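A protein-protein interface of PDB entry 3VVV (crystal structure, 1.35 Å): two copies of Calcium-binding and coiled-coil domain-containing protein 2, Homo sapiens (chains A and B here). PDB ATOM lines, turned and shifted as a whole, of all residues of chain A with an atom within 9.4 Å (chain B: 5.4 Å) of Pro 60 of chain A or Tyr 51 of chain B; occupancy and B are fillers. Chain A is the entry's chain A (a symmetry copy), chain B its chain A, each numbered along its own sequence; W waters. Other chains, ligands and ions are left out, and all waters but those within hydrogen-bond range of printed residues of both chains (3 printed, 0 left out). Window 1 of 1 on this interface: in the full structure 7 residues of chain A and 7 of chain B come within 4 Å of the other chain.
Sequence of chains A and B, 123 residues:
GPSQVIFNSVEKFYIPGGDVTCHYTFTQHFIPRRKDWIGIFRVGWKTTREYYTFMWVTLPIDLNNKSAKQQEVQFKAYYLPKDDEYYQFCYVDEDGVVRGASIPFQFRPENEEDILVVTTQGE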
ATOM      1  N   TYR A  24     -14.066 -22.268  18.590  1.00  0.00           N
ATOM      2  CA  TYR A  24     -14.939 -22.807  17.547  1.00  0.00           C
ATOM      3  C   TYR A  24     -14.843 -24.330  17.525  1.00  0.00           C
ATOM      4  O   TYR A  24     -13.869 -24.913  18.000  1.00  0.00           O
ATOM      5  CB  TYR A  24     -14.580 -22.204  16.155  1.00  0.00           C
ATOM      6  CG  TYR A  24     -13.133 -22.430  15.730  1.00  0.00           C
ATOM      7  CD1 TYR A  24     -12.120 -21.643  16.237  1.00  0.00           C
ATOM      8  CD2 TYR A  24     -12.798 -23.441  14.813  1.00  0.00           C
ATOM      9  CE1 TYR A  24     -10.797 -21.825  15.859  1.00  0.00           C
ATOM     10  CE2 TYR A  24     -11.481 -23.644  14.440  1.00  0.00           C
ATOM     11  CZ  TYR A  24     -10.488 -22.834  14.973  1.00  0.00           C
ATOM     12  OH  TYR A  24      -9.170 -23.038  14.637  1.00  0.00           O
ATOM     13  N   PHE A  26     -15.891 -27.848  14.891  1.00  0.00           N
ATOM     14  CA  PHE A  26     -16.277 -28.304  13.569  1.00  0.00           C
ATOM     15  C   PHE A  26     -17.471 -29.239  13.715  1.00  0.00           C
ATOM     16  O   PHE A  26     -17.488 -30.098  14.598  1.00  0.00           O
ATOM     17  CB  PHE A  26     -15.107 -29.072  12.950  1.00  0.00           C
ATOM     18  CG  PHE A  26     -13.847 -28.283  12.834  1.00  0.00           C
ATOM     19  CD1 PHE A  26     -13.843 -27.051  12.197  1.00  0.00           C
ATOM     20  CD2 PHE A  26     -12.665 -28.774  13.359  1.00  0.00           C
ATOM     21  CE1 PHE A  26     -12.662 -26.310  12.078  1.00  0.00           C
ATOM     22  CE2 PHE A  26     -11.498 -28.063  13.251  1.00  0.00           C
ATOM     23  CZ  PHE A  26     -11.493 -26.826  12.615  1.00  0.00           C
ATOM     24  N   PRO A  32     -12.019 -29.562   7.638  1.00  0.00           N
ATOM     25  CA  PRO A  32     -11.243 -28.329   7.575  1.00  0.00           C
ATOM     26  C   PRO A  32     -10.079 -28.516   6.604  1.00  0.00           C
ATOM     27  O   PRO A  32      -9.586 -29.637   6.438  1.00  0.00           O
ATOM     28  CB  PRO A  32     -10.695 -28.150   9.013  1.00  0.00           C
ATOM     29  CG  PRO A  32     -11.332 -29.231   9.832  1.00  0.00           C
ATOM     30  CD  PRO A  32     -11.931 -30.249   8.938  1.00  0.00           C
ATOM     31  N   ARG A  33      -9.624 -27.418   6.015  1.00  0.00           N
ATOM     32  CA  ARG A  33      -8.508 -27.417   5.093  1.00  0.00           C
ATOM     33  C   ARG A  33      -7.442 -26.420   5.527  1.00  0.00           C
ATOM     34  O   ARG A  33      -7.730 -25.486   6.279  1.00  0.00           O
ATOM     35  CB  ARG A  33      -8.978 -27.149   3.677  1.00  0.00           C
ATOM     36  CG  ARG A  33      -9.780 -28.288   3.091  1.00  0.00           C
ATOM     37  CD  ARG A  33     -10.291 -27.971   1.709  1.00  0.00           C
ATOM     38  NE  ARG A  33     -11.471 -27.111   1.817  1.00  0.00           N
ATOM     39  CZ  ARG A  33     -12.091 -26.581   0.769  1.00  0.00           C
ATOM     40  NH1 ARG A  33     -11.612 -26.780  -0.470  1.00  0.00           N
ATOM     41  NH2 ARG A  33     -13.174 -25.826   0.945  1.00  0.00           N
ATOM     42  N   ARG A  34      -6.204 -26.620   5.081  1.00  0.00           N
ATOM     43  CA  ARG A  34      -5.047 -25.933   5.667  1.00  0.00           C
ATOM     44  C   ARG A  34      -5.028 -24.416   5.421  1.00  0.00           C
ATOM     45  O   ARG A  34      -4.421 -23.694   6.162  1.00  0.00           O
ATOM     46  CB  ARG A  34      -3.712 -26.546   5.181  1.00  0.00           C
ATOM     47  CG  ARG A  34      -3.573 -28.075   5.243  1.00  0.00           C
ATOM     48  CD  ARG A  34      -3.412 -28.608   6.640  1.00  0.00           C
ATOM     49  NE  ARG A  34      -3.343 -30.071   6.629  1.00  0.00           N
ATOM     50  CZ  ARG A  34      -2.224 -30.791   6.544  1.00  0.00           C
ATOM     51  NH1 ARG A  34      -1.049 -30.210   6.471  1.00  0.00           N
ATOM     52  NH2 ARG A  34      -2.310 -32.121   6.507  1.00  0.00           N
ATOM     53  N   VAL A  57      -6.694 -20.987  10.269  1.00  0.00           N
ATOM     54  CA  VAL A  57      -7.268 -22.006  11.144  1.00  0.00           C
ATOM     55  C   VAL A  57      -6.160 -22.696  11.946  1.00  0.00           C
ATOM     56  O   VAL A  57      -5.069 -22.999  11.430  1.00  0.00           O
ATOM     57  CB  VAL A  57      -8.135 -23.017  10.332  1.00  0.00           C
ATOM     58  CG1 VAL A  57      -7.287 -23.858   9.369  1.00  0.00           C
ATOM     59  CG2 VAL A  57      -8.916 -23.922  11.249  1.00  0.00           C
ATOM     60  N   THR A  58      -6.391 -22.943  13.236  1.00  0.00           N
ATOM     61  CA  THR A  58      -5.364 -23.576  14.072  1.00  0.00           C
ATOM     62  C   THR A  58      -5.028 -24.986  13.584  1.00  0.00           C
ATOM     63  O   THR A  58      -5.932 -25.791  13.288  1.00  0.00           O
ATOM     64  CB  THR A  58      -5.828 -23.618  15.529  1.00  0.00           C
ATOM     65  OG1 THR A  58      -5.888 -22.262  15.984  1.00  0.00           O
ATOM     66  CG2 THR A  58      -4.850 -24.443  16.402  1.00  0.00           C
ATOM     67  N   LEU A  59      -3.733 -25.279  13.507  1.00  0.00           N
ATOM     68  CA  LEU A  59      -3.253 -26.618  13.160  1.00  0.00           C
ATOM     69  C   LEU A  59      -2.299 -27.085  14.241  1.00  0.00           C
ATOM     70  O   LEU A  59      -1.776 -26.270  15.000  1.00  0.00           O
ATOM     71  CB  LEU A  59      -2.492 -26.556  11.828  1.00  0.00           C
ATOM     72  CG  LEU A  59      -3.325 -26.247  10.582  1.00  0.00           C
ATOM     73  CD1 LEU A  59      -2.442 -26.228   9.325  1.00  0.00           C
ATOM     74  CD2 LEU A  59      -4.524 -27.205  10.420  1.00  0.00           C
ATOM     75  N   PRO A  60      -2.053 -28.397  14.320  1.00  0.00           N
ATOM     76  CA  PRO A  60      -2.718 -29.468  13.566  1.00  0.00           C
ATOM     77  C   PRO A  60      -4.127 -29.730  14.087  1.00  0.00           C
ATOM     78  O   PRO A  60      -4.510 -29.249  15.146  1.00  0.00           O
ATOM     79  CB  PRO A  60      -1.803 -30.683  13.764  1.00  0.00           C
ATOM     80  CG  PRO A  60      -1.200 -30.452  15.127  1.00  0.00           C
ATOM     81  CD  PRO A  60      -1.043 -28.919  15.268  1.00  0.00           C
ATOM     82  N   ILE A  61      -4.899 -30.485  13.319  1.00  0.00           N
ATOM     83  CA  ILE A  61      -6.250 -30.858  13.700  1.00  0.00           C
ATOM     84  C   ILE A  61      -6.372 -32.382  13.765  1.00  0.00           C
ATOM     85  O   ILE A  61      -5.981 -33.081  12.822  1.00  0.00           O
ATOM     86  CB  ILE A  61      -7.261 -30.297  12.691  1.00  0.00           C
ATOM     87  CG1 ILE A  61      -7.297 -28.761  12.750  1.00  0.00           C
ATOM     88  CG2 ILE A  61      -8.633 -30.837  12.970  1.00  0.00           C
ATOM     89  CD1 ILE A  61      -7.949 -28.129  11.544  1.00  0.00           C
ATOM     90  N   ASP A  62      -6.928 -32.879  14.869  1.00  0.00           N
ATOM     91  CA  ASP A  62      -7.078 -34.317  15.090  1.00  0.00           C
ATOM     92  C   ASP A  62      -7.587 -35.016  13.849  1.00  0.00           C
ATOM     93  O   ASP A  62      -8.664 -34.715  13.365  1.00  0.00           O
ATOM     94  CB  ASP A  62      -8.005 -34.585  16.279  1.00  0.00           C
ATOM     95  CG  ASP A  62      -7.306 -34.400  17.618  1.00  0.00           C
ATOM     96  OD1 ASP A  62      -6.133 -34.816  17.735  1.00  0.00           O
ATOM     97  OD2 ASP A  62      -7.925 -33.841  18.550  1.00  0.00           O
ATOM     98  N   LYS A  69     -13.992 -31.861  19.408  1.00  0.00           N
ATOM     99  CA  LYS A  69     -12.852 -31.300  20.116  1.00  0.00           C
ATOM    100  C   LYS A  69     -12.866 -29.775  19.963  1.00  0.00           C
ATOM    101  O   LYS A  69     -13.081 -29.230  18.858  1.00  0.00           O
ATOM    102  CB  LYS A  69     -11.528 -31.900  19.612  1.00  0.00           C
ATOM    103  N   GLN A  70     -12.648 -29.089  21.078  1.00  0.00           N
ATOM    104  CA  GLN A  70     -12.606 -27.631  21.087  1.00  0.00           C
ATOM    105  C   GLN A  70     -11.426 -27.144  20.275  1.00  0.00           C
ATOM    106  O   GLN A  70     -10.339 -27.723  20.361  1.00  0.00           O
ATOM    107  CB  GLN A  70     -12.479 -27.121  22.526  1.00  0.00           C
ATOM    108  CG  GLN A  70     -13.795 -27.055  23.288  1.00  0.00           C
ATOM    109  CD  GLN A  70     -14.624 -25.835  22.910  1.00  0.00           C
ATOM    110  OE1 GLN A  70     -14.437 -25.247  21.846  1.00  0.00           O
ATOM    111  NE2 GLN A  70     -15.531 -25.439  23.794  1.00  0.00           N
ATOM    112  N   GLN A  71     -11.637 -26.094  19.476  1.00  0.00           N
ATOM    113  CA  GLN A  71     -10.539 -25.435  18.785  1.00  0.00           C
ATOM    114  C   GLN A  71     -10.500 -24.010  19.264  1.00  0.00           C
ATOM    115  O   GLN A  71     -11.519 -23.451  19.700  1.00  0.00           O
ATOM    116  CB  GLN A  71     -10.740 -25.388  17.267  1.00  0.00           C
ATOM    117  CG  GLN A  71     -11.010 -26.716  16.611  1.00  0.00           C
ATOM    118  CD  GLN A  71      -9.831 -27.651  16.695  1.00  0.00           C
ATOM    119  OE1 GLN A  71      -8.715 -27.297  16.300  1.00  0.00           O
ATOM    120  NE2 GLN A  71     -10.061 -28.852  17.206  1.00  0.00           N
ATOM    121  N   GLU A  72      -9.339 -23.389  19.194  1.00  0.00           N
ATOM    122  CA  GLU A  72      -9.296 -21.975  19.457  1.00  0.00           C
ATOM    123  C   GLU A  72      -8.193 -21.348  18.659  1.00  0.00           C
ATOM    124  O   GLU A  72      -7.257 -22.034  18.234  1.00  0.00           O
ATOM    125  CB  GLU A  72      -9.114 -21.689  20.942  1.00  0.00           C
ATOM    126  CG  GLU A  72      -7.867 -22.235  21.542  1.00  0.00           C
ATOM    127  CD  GLU A  72      -7.905 -22.092  23.072  1.00  0.00           C
ATOM    128  OE1 GLU A  72      -7.260 -21.162  23.577  1.00  0.00           O
ATOM    129  OE2 GLU A  72      -8.587 -22.892  23.767  1.00  0.00           O
ATOM    130  N   TRP B  37       3.939 -31.243  18.953  1.00  0.00           N
ATOM    131  CA  TRP B  37       3.577 -32.348  18.081  1.00  0.00           C
ATOM    132  C   TRP B  37       4.716 -32.753  17.196  1.00  0.00           C
ATOM    133  O   TRP B  37       5.688 -32.023  17.020  1.00  0.00           O
ATOM    134  CB  TRP B  37       2.336 -31.988  17.254  1.00  0.00           C
ATOM    135  CG  TRP B  37       2.386 -30.673  16.497  1.00  0.00           C
ATOM    136  CD1 TRP B  37       2.167 -29.419  17.020  1.00  0.00           C
ATOM    137  CD2 TRP B  37       2.612 -30.496  15.086  1.00  0.00           C
ATOM    138  NE1 TRP B  37       2.270 -28.478  16.018  1.00  0.00           N
ATOM    139  CE2 TRP B  37       2.496 -29.116  14.821  1.00  0.00           C
ATOM    140  CE3 TRP B  37       2.889 -31.373  14.025  1.00  0.00           C
ATOM    141  CZ2 TRP B  37       2.654 -28.583  13.543  1.00  0.00           C
ATOM    142  CZ3 TRP B  37       3.037 -30.825  12.727  1.00  0.00           C
ATOM    143  CH2 TRP B  37       2.911 -29.449  12.514  1.00  0.00           C
ATOM    144  N   GLY B  39       5.368 -33.994  13.294  1.00  0.00           N
ATOM    145  CA  GLY B  39       4.854 -34.205  11.959  1.00  0.00           C
ATOM    146  C   GLY B  39       5.781 -35.053  11.112  1.00  0.00           C
ATOM    147  O   GLY B  39       7.001 -35.092  11.334  1.00  0.00           O
ATOM    148  N   ILE B  40       5.177 -35.683  10.113  1.00  0.00           N
ATOM    149  CA  ILE B  40       5.931 -36.233   9.000  1.00  0.00           C
ATOM    150  C   ILE B  40       5.767 -35.239   7.855  1.00  0.00           C
ATOM    151  O   ILE B  40       4.636 -34.918   7.456  1.00  0.00           O
ATOM    152  CB  ILE B  40       5.398 -37.633   8.610  1.00  0.00           C
ATOM    153  CG1 ILE B  40       5.665 -38.640   9.731  1.00  0.00           C
ATOM    154  CG2 ILE B  40       6.051 -38.086   7.272  1.00  0.00           C
ATOM    155  CD1 ILE B  40       5.061 -40.025   9.462  1.00  0.00           C
ATOM    156  N   PHE B  41       6.902 -34.727   7.374  1.00  0.00           N
ATOM    157  CA  PHE B  41       6.954 -33.656   6.392  1.00  0.00           C
ATOM    158  C   PHE B  41       7.734 -34.113   5.180  1.00  0.00           C
ATOM    159  O   PHE B  41       8.724 -34.833   5.313  1.00  0.00           O
ATOM    160  CB  PHE B  41       7.732 -32.472   6.978  1.00  0.00           C
ATOM    161  CG  PHE B  41       6.954 -31.649   7.978  1.00  0.00           C
ATOM    162  CD1 PHE B  41       6.208 -30.557   7.557  1.00  0.00           C
ATOM    163  CD2 PHE B  41       6.970 -31.980   9.329  1.00  0.00           C
ATOM    164  CE1 PHE B  41       5.511 -29.792   8.498  1.00  0.00           C
ATOM    165  CE2 PHE B  41       6.275 -31.212  10.267  1.00  0.00           C
ATOM    166  CZ  PHE B  41       5.551 -30.131   9.851  1.00  0.00           C
ATOM    167  N   THR B  47       6.516 -24.476   5.394  1.00  0.00           N
ATOM    168  CA  THR B  47       5.880 -24.050   6.645  1.00  0.00           C
ATOM    169  C   THR B  47       5.369 -25.279   7.370  1.00  0.00           C
ATOM    170  O   THR B  47       5.114 -26.328   6.751  1.00  0.00           O
ATOM    171  CB  THR B  47       4.713 -23.088   6.415  1.00  0.00           C
ATOM    172  OG1 THR B  47       3.562 -23.842   6.042  1.00  0.00           O
ATOM    173  CG2 THR B  47       5.050 -22.070   5.329  1.00  0.00           C
ATOM    174  N   THR B  48       5.202 -25.158   8.686  1.00  0.00           N
ATOM    175  CA  THR B  48       4.761 -26.301   9.493  1.00  0.00           C
ATOM    176  C   THR B  48       3.328 -26.702   9.170  1.00  0.00           C
ATOM    177  O   THR B  48       2.876 -27.768   9.570  1.00  0.00           O
ATOM    178  CB  THR B  48       4.876 -26.044  10.981  1.00  0.00           C
ATOM    179  OG1 THR B  48       4.129 -24.863  11.299  1.00  0.00           O
ATOM    180  CG2 THR B  48       6.344 -25.857  11.406  1.00  0.00           C
ATOM    181  N   ARG B  49       2.622 -25.843   8.437  1.00  0.00           N
ATOM    182  CA  ARG B  49       1.252 -26.128   8.046  1.00  0.00           C
ATOM    183  C   ARG B  49       1.164 -27.188   6.944  1.00  0.00           C
ATOM    184  O   ARG B  49       0.088 -27.618   6.608  1.00  0.00           O
ATOM    185  CB  ARG B  49       0.530 -24.855   7.609  1.00  0.00           C
ATOM    186  CG  ARG B  49       0.478 -23.794   8.715  1.00  0.00           C
ATOM    187  CD  ARG B  49      -0.336 -22.579   8.308  1.00  0.00           C
ATOM    188  NE  ARG B  49      -1.757 -22.876   8.106  1.00  0.00           N
ATOM    189  CZ  ARG B  49      -2.654 -22.886   9.097  1.00  0.00           C
ATOM    190  NH1 ARG B  49      -2.276 -22.668  10.362  1.00  0.00           N
ATOM    191  NH2 ARG B  49      -3.930 -23.138   8.832  1.00  0.00           N
ATOM    192  N   GLU B  50       2.313 -27.593   6.411  1.00  0.00           N
ATOM    193  CA  GLU B  50       2.418 -28.543   5.302  1.00  0.00           C
ATOM    194  C   GLU B  50       2.583 -29.993   5.712  1.00  0.00           C
ATOM    195  O   GLU B  50       2.876 -30.833   4.856  1.00  0.00           O
ATOM    196  CB  GLU B  50       3.587 -28.159   4.384  1.00  0.00           C
ATOM    197  CG  GLU B  50       3.394 -26.814   3.734  1.00  0.00           C
ATOM    198  CD  GLU B  50       4.608 -26.329   2.976  1.00  0.00           C
ATOM    199  OE1 GLU B  50       5.544 -27.101   2.721  1.00  0.00           O
ATOM    200  OE2 GLU B  50       4.618 -25.153   2.659  1.00  0.00           O
ATOM    201  N   TYR B  51       2.437 -30.330   6.981  1.00  0.00           N
ATOM    202  CA  TYR B  51       2.683 -31.702   7.401  1.00  0.00           C
ATOM    203  C   TYR B  51       1.840 -32.680   6.606  1.00  0.00           C
ATOM    204  O   TYR B  51       0.703 -32.382   6.250  1.00  0.00           O
ATOM    205  CB  TYR B  51       2.408 -31.859   8.916  1.00  0.00           C
ATOM    206  CG  TYR B  51       0.970 -31.553   9.339  1.00  0.00           C
ATOM    207  CD1 TYR B  51       0.582 -30.267   9.718  1.00  0.00           C
ATOM    208  CD2 TYR B  51      -0.002 -32.550   9.354  1.00  0.00           C
ATOM    209  CE1 TYR B  51      -0.712 -30.002  10.101  1.00  0.00           C
ATOM    210  CE2 TYR B  51      -1.332 -32.274   9.720  1.00  0.00           C
ATOM    211  CZ  TYR B  51      -1.658 -30.993  10.091  1.00  0.00           C
ATOM    212  OH  TYR B  51      -2.955 -30.678  10.480  1.00  0.00           O
ATOM    213  N   TYR B  52       2.376 -33.863   6.342  1.00  0.00           N
ATOM    214  CA  TYR B  52       1.592 -34.916   5.705  1.00  0.00           C
ATOM    215  C   TYR B  52       0.637 -35.538   6.721  1.00  0.00           C
ATOM    216  O   TYR B  52      -0.554 -35.703   6.458  1.00  0.00           O
ATOM    217  CB  TYR B  52       2.527 -35.991   5.128  1.00  0.00           C
ATOM    218  CG  TYR B  52       1.776 -36.955   4.244  1.00  0.00           C
ATOM    219  CD1 TYR B  52       1.114 -38.045   4.780  1.00  0.00           C
ATOM    220  CD2 TYR B  52       1.656 -36.732   2.863  1.00  0.00           C
ATOM    221  CE1 TYR B  52       0.386 -38.908   4.004  1.00  0.00           C
ATOM    222  CE2 TYR B  52       0.922 -37.617   2.060  1.00  0.00           C
ATOM    223  CZ  TYR B  52       0.297 -38.694   2.647  1.00  0.00           C
ATOM    224  OH  TYR B  52      -0.448 -39.572   1.875  1.00  0.00           O
ATOM    225  N   THR B  53       1.167 -35.859   7.894  1.00  0.00           N
ATOM    226  CA  THR B  53       0.357 -36.332   9.007  1.00  0.00           C
ATOM    227  C   THR B  53       1.108 -35.952  10.284  1.00  0.00           C
ATOM    228  O   THR B  53       2.229 -35.434  10.222  1.00  0.00           O
ATOM    229  CB  THR B  53       0.069 -37.851   8.935  1.00  0.00           C
ATOM    230  OG1 THR B  53      -0.906 -38.170   9.927  1.00  0.00           O
ATOM    231  CG2 THR B  53       1.359 -38.664   9.171  1.00  0.00           C
ATOM    232  N   PHE B  54       0.520 -36.209  11.447  1.00  0.00           N
ATOM    233  CA  PHE B  54       1.128 -35.773  12.699  1.00  0.00           C
ATOM    234  C   PHE B  54       0.621 -36.651  13.838  1.00  0.00           C
ATOM    235  O   PHE B  54      -0.403 -37.335  13.707  1.00  0.00           O
ATOM    236  CB  PHE B  54       0.772 -34.292  13.013  1.00  0.00           C
ATOM    237  CG  PHE B  54      -0.576 -34.144  13.650  1.00  0.00           C
ATOM    238  CD1 PHE B  54      -1.732 -34.261  12.884  1.00  0.00           C
ATOM    239  CD2 PHE B  54      -0.706 -33.993  15.029  1.00  0.00           C
ATOM    240  CE1 PHE B  54      -2.989 -34.198  13.481  1.00  0.00           C
ATOM    241  CE2 PHE B  54      -1.983 -33.923  15.616  1.00  0.00           C
ATOM    242  CZ  PHE B  54      -3.103 -34.026  14.850  1.00  0.00           C
ATOM    243  N   TRP B  56       0.245 -35.793  18.243  1.00  0.00           N
ATOM    244  CA  TRP B  56       0.601 -34.957  19.399  1.00  0.00           C
ATOM    245  C   TRP B  56       1.720 -35.638  20.180  1.00  0.00           C
ATOM    246  O   TRP B  56       1.798 -36.876  20.217  1.00  0.00           O
ATOM    247  CB  TRP B  56      -0.600 -34.783  20.341  1.00  0.00           C
ATOM    248  CG  TRP B  56      -1.782 -34.090  19.699  1.00  0.00           C
ATOM    249  CD1 TRP B  56      -2.970 -34.670  19.344  1.00  0.00           C
ATOM    250  CD2 TRP B  56      -1.870 -32.704  19.308  1.00  0.00           C
ATOM    251  NE1 TRP B  56      -3.800 -33.730  18.784  1.00  0.00           N
ATOM    252  CE2 TRP B  56      -3.156 -32.521  18.749  1.00  0.00           C
ATOM    253  CE3 TRP B  56      -1.014 -31.600  19.415  1.00  0.00           C
ATOM    254  CZ2 TRP B  56      -3.600 -31.294  18.270  1.00  0.00           C
ATOM    255  CZ3 TRP B  56      -1.467 -30.367  18.928  1.00  0.00           C
ATOM    256  CH2 TRP B  56      -2.742 -30.234  18.367  1.00  0.00           C
HETATM  257  O   HOH W   1      -1.936 -22.922  13.722  1.00  0.00           O
HETATM  258  O   HOH W   2      -4.861 -32.659   9.962  1.00  0.00           O
HETATM  259  O   HOH W   3      -1.463 -23.193   5.139  1.00  0.00           O
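Pro 60 of chain A touches just these residues of chain B: Trp 37 (3.4 Å), Tyr 51 (3.3 Å), Phe 54 (3.6 Å) and Trp 56 (3.6 Å). Of the printed residues of chain B, Arg 34 of chain A touches Arg 49, Glu 50, Tyr 51 and Tyr 52. Of the printed residues of chain B, Leu 59 of chain A touches Arg 49 (3.4 Å) and Tyr 51 (3.8 Å). Of the printed residues of chain B, Val 57 of chain A touches Arg 49 (2.8 Å). Printed residues of chain A within 4 Å of Tyr 52 of chain B: Arg 34 (3.99 Å). Thr 48 of chain B touches none of the printed residues of chain A. Lys 69 of chain A touches none of the printed residues of chain B.
NH2 of Arg 49 of chain B is in hydrogen-bond range of O of Arg 34 of chain A (2.8 Å). The guanidinium group of Arg 49 of chain B lies within hydrogen-bond range of the backbone carbonyl oxygen of Val 57 of chain A (2.8 Å). O of Tyr 51 of chain B is in hydrogen-bond range of NH1 of Arg 34 of chain A (2.8 Å). OH of Tyr 51 of chain B lies within hydrogen-bond range of N of Ile 61 of chain A, 3.4 Å away. NE1 of Trp 56 of chain B is in hydrogen-bond range of OD1 of Asp 62 of chain A (2.8 Å).
Water W2 bridges the side-chain hydroxyl (OH) of Tyr 51 of chain B (2.8 Å) and the backbone carbonyl oxygen (O) of Ile 61 of chain A (3.1 Å). Water W1 bridges the backbone NH of Leu 59 of chain A (3.0 Å) and the guanidinium group of Arg 49 of chain B (3.4 Å). Water W3 bridges the guanidinium group of Arg 49 of chain B (3.0 Å) and the backbone carbonyl oxygen of Arg 34 of chain A (3.2 Å).
NH1 of Arg 34 of chain A touches C of Glu 50 of chain B, 3.7 Å away. Arg 34 of chain A touches Tyr 52 of chain B (NH2 to O, 3.99 Å). Arg 49 of chain B touches Leu 59 of chain A. OH of Tyr 51 of chain B touches CD2 of Leu 59 of chain A, at 3.8 Å. NE1 of Trp 37 of chain B touches CD of Pro 60 of chain A (3.4 Å). Pro 60 of chain A touches Tyr 51 of chain B (CA to OH, 3.3 Å). Pro 60 of chain A touches Phe 54 of chain B (CG to CD2, 3.6 Å). Pro 60 of chain A touches Trp 56 of chain B (CG to CH2, 3.6 Å). Phe 54 of chain B touches Ile 61 of chain A. Asp 62 of chain A touches Phe 54 of chain B.
Hydrophobic or aromatic side chains of chain B that line the printed part of chain A: Trp 37, Tyr 51, Phe 54 and Trp 56. Along chain B the printed residues that touch a printed residue of chain A span positions 37 to 56. Among the printed residues, no Asp or Glu carboxylate lies within 4 Å of a Lys or Arg side-chain nitrogen of the other chain.
The backbone carbonyl oxygen of Ile 40 of chain B is in hydrogen-bond range of the backbone NH of Tyr 52 of chain B. The backbone NH of Arg 49 of chain B lies close to the side-chain hydroxyl of Thr 47 of chain B, at 3.3 Å. N of Thr 47 of chain B sits at hydrogen-bond distance from OE2 of Glu 50 of chain B (3.4 Å).
No position is printed for both chains. Of the 15 pairs that touch across the chains among the printed residues, none has its exchanged pair printed and touching as well.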
